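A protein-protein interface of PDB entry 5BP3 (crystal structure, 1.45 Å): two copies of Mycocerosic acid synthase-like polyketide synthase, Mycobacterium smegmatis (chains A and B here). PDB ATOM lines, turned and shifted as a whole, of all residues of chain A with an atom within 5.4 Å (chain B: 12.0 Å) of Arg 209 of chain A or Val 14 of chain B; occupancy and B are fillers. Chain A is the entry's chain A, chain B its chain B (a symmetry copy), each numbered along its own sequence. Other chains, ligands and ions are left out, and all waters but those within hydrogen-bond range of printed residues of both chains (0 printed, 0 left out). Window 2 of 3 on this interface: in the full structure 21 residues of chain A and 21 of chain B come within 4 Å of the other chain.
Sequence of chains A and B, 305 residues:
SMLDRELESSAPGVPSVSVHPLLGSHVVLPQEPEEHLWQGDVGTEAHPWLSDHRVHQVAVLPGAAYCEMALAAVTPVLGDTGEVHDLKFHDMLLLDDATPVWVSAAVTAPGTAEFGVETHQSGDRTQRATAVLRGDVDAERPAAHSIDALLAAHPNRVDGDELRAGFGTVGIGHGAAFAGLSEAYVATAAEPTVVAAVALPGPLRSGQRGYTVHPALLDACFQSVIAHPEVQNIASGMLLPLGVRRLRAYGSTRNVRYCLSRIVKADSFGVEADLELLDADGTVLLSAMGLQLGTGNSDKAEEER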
ATOM      1  N   SER A  18      19.521 -15.599  27.247  1.00  0.00           N
ATOM      2  CA  SER A  18      20.106 -14.702  26.262  1.00  0.00           C
ATOM      3  C   SER A  18      21.516 -15.208  25.944  1.00  0.00           C
ATOM      4  O   SER A  18      22.176 -15.809  26.804  1.00  0.00           O
ATOM      5  CB  SER A  18      20.092 -13.270  26.779  1.00  0.00           C
ATOM      6  OG  SER A  18      20.515 -13.224  28.122  1.00  0.00           O
ATOM      7  N   VAL A  19      21.957 -15.014  24.697  1.00  0.00           N
ATOM      8  CA  VAL A  19      23.280 -15.451  24.290  1.00  0.00           C
ATOM      9  C   VAL A  19      23.929 -14.347  23.483  1.00  0.00           C
ATOM     10  O   VAL A  19      23.251 -13.521  22.874  1.00  0.00           O
ATOM     11  CB  VAL A  19      23.267 -16.717  23.429  1.00  0.00           C
ATOM     12  CG1 VAL A  19      22.714 -17.912  24.225  1.00  0.00           C
ATOM     13  CG2 VAL A  19      22.438 -16.528  22.198  1.00  0.00           C
ATOM     14  N   PRO A  21      25.655 -13.091  20.248  1.00  0.00           N
ATOM     15  CA  PRO A  21      25.318 -13.526  18.883  1.00  0.00           C
ATOM     16  C   PRO A  21      26.328 -14.457  18.206  1.00  0.00           C
ATOM     17  O   PRO A  21      25.933 -15.256  17.347  1.00  0.00           O
ATOM     18  CB  PRO A  21      25.233 -12.211  18.103  1.00  0.00           C
ATOM     19  CG  PRO A  21      24.905 -11.192  19.094  1.00  0.00           C
ATOM     20  CD  PRO A  21      25.489 -11.640  20.415  1.00  0.00           C
ATOM     21  N   ARG A 205      22.007  -1.825  12.599  1.00  0.00           N
ATOM     22  CA  ARG A 205      21.883  -1.132  13.874  1.00  0.00           C
ATOM     23  C   ARG A 205      20.876  -1.797  14.805  1.00  0.00           C
ATOM     24  O   ARG A 205      21.010  -1.710  16.024  1.00  0.00           O
ATOM     25  CB  ARG A 205      21.550   0.349  13.675  1.00  0.00           C
ATOM     26  CG  ARG A 205      22.730   1.139  13.131  1.00  0.00           C
ATOM     27  CD  ARG A 205      22.581   2.644  13.322  1.00  0.00           C
ATOM     28  NE  ARG A 205      23.849   3.311  13.069  1.00  0.00           N
ATOM     29  CZ  ARG A 205      24.817   3.455  13.972  1.00  0.00           C
ATOM     30  NH1 ARG A 205      24.667   2.992  15.214  1.00  0.00           N
ATOM     31  NH2 ARG A 205      25.939   4.069  13.631  1.00  0.00           N
ATOM     32  N   SER A 206      19.886  -2.482  14.244  1.00  0.00           N
ATOM     33  CA  SER A 206      18.909  -3.175  15.073  1.00  0.00           C
ATOM     34  C   SER A 206      19.561  -4.353  15.809  1.00  0.00           C
ATOM     35  O   SER A 206      19.236  -4.633  16.965  1.00  0.00           O
ATOM     36  CB  SER A 206      17.733  -3.670  14.228  1.00  0.00           C
ATOM     37  OG  SER A 206      18.020  -4.928  13.636  1.00  0.00           O
ATOM     38  N   GLY A 207      20.497  -5.024  15.141  1.00  0.00           N
ATOM     39  CA  GLY A 207      21.074  -6.250  15.659  1.00  0.00           C
ATOM     40  C   GLY A 207      22.387  -6.095  16.409  1.00  0.00           C
ATOM     41  O   GLY A 207      23.040  -7.096  16.707  1.00  0.00           O
ATOM     42  N   GLN A 208      22.782  -4.864  16.729  1.00  0.00           N
ATOM     43  CA  GLN A 208      24.058  -4.652  17.422  1.00  0.00           C
ATOM     44  C   GLN A 208      23.899  -4.815  18.938  1.00  0.00           C
ATOM     45  O   GLN A 208      24.867  -4.657  19.698  1.00  0.00           O
ATOM     46  CB  GLN A 208      24.677  -3.294  17.064  1.00  0.00           C
ATOM     47  CG  GLN A 208      23.943  -2.090  17.611  1.00  0.00           C
ATOM     48  CD  GLN A 208      24.639  -0.777  17.266  1.00  0.00           C
ATOM     49  OE1 GLN A 208      23.985   0.191  16.865  1.00  0.00           O
ATOM     50  NE2 GLN A 208      25.970  -0.736  17.424  1.00  0.00           N
ATOM     51  N   ARG A 209      22.671  -5.144  19.356  1.00  0.00           N
ATOM     52  CA  ARG A 209      22.372  -5.490  20.742  1.00  0.00           C
ATOM     53  C   ARG A 209      23.096  -6.777  21.129  1.00  0.00           C
ATOM     54  O   ARG A 209      22.920  -7.846  20.527  1.00  0.00           O
ATOM     55  CB  ARG A 209      20.862  -5.648  20.975  1.00  0.00           C
ATOM     56  N   GLY A 210      23.914  -6.661  22.155  1.00  0.00           N
ATOM     57  CA  GLY A 210      24.639  -7.800  22.654  1.00  0.00           C
ATOM     58  C   GLY A 210      26.088  -7.732  22.215  1.00  0.00           C
ATOM     59  O   GLY A 210      26.904  -8.449  22.792  1.00  0.00           O
ATOM     60  N   TYR A 211      26.435  -6.899  21.229  1.00  0.00           N
ATOM     61  CA  TYR A 211      27.828  -6.840  20.875  1.00  0.00           C
ATOM     62  C   TYR A 211      28.589  -5.823  21.729  1.00  0.00           C
ATOM     63  O   TYR A 211      28.066  -4.756  22.011  1.00  0.00           O
ATOM     64  CB  TYR A 211      28.005  -6.415  19.413  1.00  0.00           C
ATOM     65  CG  TYR A 211      27.658  -7.491  18.406  1.00  0.00           C
ATOM     66  CD1 TYR A 211      28.472  -8.587  18.235  1.00  0.00           C
ATOM     67  CD2 TYR A 211      26.523  -7.396  17.619  1.00  0.00           C
ATOM     68  CE1 TYR A 211      28.171  -9.559  17.301  1.00  0.00           C
ATOM     69  CE2 TYR A 211      26.198  -8.389  16.702  1.00  0.00           C
ATOM     70  CZ  TYR A 211      27.032  -9.451  16.551  1.00  0.00           C
ATOM     71  OH  TYR A 211      26.760 -10.409  15.625  1.00  0.00           O
ATOM     72  N   VAL B  14      18.487  -8.591  21.356  1.00  0.00           N
ATOM     73  CA  VAL B  14      19.438  -9.589  21.859  1.00  0.00           C
ATOM     74  C   VAL B  14      18.935 -11.021  21.611  1.00  0.00           C
ATOM     75  O   VAL B  14      17.831 -11.373  22.008  1.00  0.00           O
ATOM     76  CB  VAL B  14      19.746  -9.394  23.378  1.00  0.00           C
ATOM     77  CG1 VAL B  14      18.462  -9.467  24.230  1.00  0.00           C
ATOM     78  CG2 VAL B  14      20.800 -10.415  23.864  1.00  0.00           C
ATOM     79  N   PRO B  15      19.756 -11.850  20.952  1.00  0.00           N
ATOM     80  CA  PRO B  15      19.288 -13.205  20.671  1.00  0.00           C
ATOM     81  C   PRO B  15      19.188 -14.075  21.921  1.00  0.00           C
ATOM     82  O   PRO B  15      19.821 -13.841  22.961  1.00  0.00           O
ATOM     83  CB  PRO B  15      20.345 -13.765  19.720  1.00  0.00           C
ATOM     84  CG  PRO B  15      21.562 -12.959  19.990  1.00  0.00           C
ATOM     85  CD  PRO B  15      21.117 -11.612  20.438  1.00  0.00           C
ATOM     86  N   SER B  16      18.366 -15.100  21.805  1.00  0.00           N
ATOM     87  CA  SER B  16      18.228 -16.040  22.892  1.00  0.00           C
ATOM     88  C   SER B  16      18.066 -17.440  22.324  1.00  0.00           C
ATOM     89  O   SER B  16      17.848 -17.616  21.127  1.00  0.00           O
ATOM     90  CB  SER B  16      17.041 -15.641  23.763  1.00  0.00           C
ATOM     91  OG  SER B  16      15.872 -15.499  22.975  1.00  0.00           O
ATOM     92  N   VAL B  17      18.170 -18.438  23.199  1.00  0.00           N
ATOM     93  CA  VAL B  17      18.073 -19.829  22.798  1.00  0.00           C
ATOM     94  C   VAL B  17      17.179 -20.530  23.815  1.00  0.00           C
ATOM     95  O   VAL B  17      17.287 -20.278  25.014  1.00  0.00           O
ATOM     96  CB  VAL B  17      19.456 -20.505  22.767  1.00  0.00           C
ATOM     97  CG1 VAL B  17      19.347 -21.953  22.346  1.00  0.00           C
ATOM     98  CG2 VAL B  17      20.386 -19.768  21.805  1.00  0.00           C
ATOM     99  N   SER B  18      16.283 -21.390  23.341  1.00  0.00           N
ATOM    100  CA  SER B  18      15.404 -22.117  24.243  1.00  0.00           C
ATOM    101  C   SER B  18      16.266 -23.132  24.979  1.00  0.00           C
ATOM    102  O   SER B  18      17.224 -23.668  24.410  1.00  0.00           O
ATOM    103  CB  SER B  18      14.278 -22.801  23.474  1.00  0.00           C
ATOM    104  OG  SER B  18      14.805 -23.545  22.386  1.00  0.00           O
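Position printed for both chains: 18. Of the 5 pairs that touch across the chains among the printed residues, none has its exchanged pair printed and touching as well.
Of the 5 printed residues of chain B, 3 touch a printed residue of chain A. Hydrophobic or aromatic side chains of chain B that line the printed part of chain A: Pro 15 and Val 17. Among the printed residues, no Asp or Glu carboxylate lies within 4 Å of a Lys or Arg side-chain nitrogen of the other chain.
Of the printed residues of chain B, Val 19 of chain A touches Pro 15 and Val 17. Printed residues of chain B within 4 Å of Pro 21 of chain A: Pro 15. Gly 207 of chain A touches none of the printed residues of chain B. No residue of chain B comes within 4 Å of Gln 208 of chain A. Printed residues of chain A within 4 Å of Val 14 of chain B: Arg 209 (3.8 Å). Of the printed residues of chain A, Pro 15 of chain B touches Ser 18, Val 19 and Pro 21. Ser 16 of chain B touches none of the printed residues of chain A. Of the printed residues of chain A, Val 17 of chain B touches Val 19 (3.8 Å). Ser 18 of chain B touches none of the printed residues of chain A. The nearest printed residue of chain A that does not touch Pro 15 of chain B is Arg 209 of chain A (4.2 Å).
The backbone NH (N) of Val 19 of chain A is in hydrogen-bond range of the backbone carbonyl oxygen (O) of Pro 15 of chain B.
Pro 15 of chain B touches Ser 18 of chain A. Val 17 of chain B touches Val 19 of chain A (CG2 to CG1, 3.8 Å). CG of Pro 21 of chain A touches CG of Pro 15 of chain B (3.9 Å). Val 14 of chain B touches Arg 209 of chain A (N to CB, 3.8 Å).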
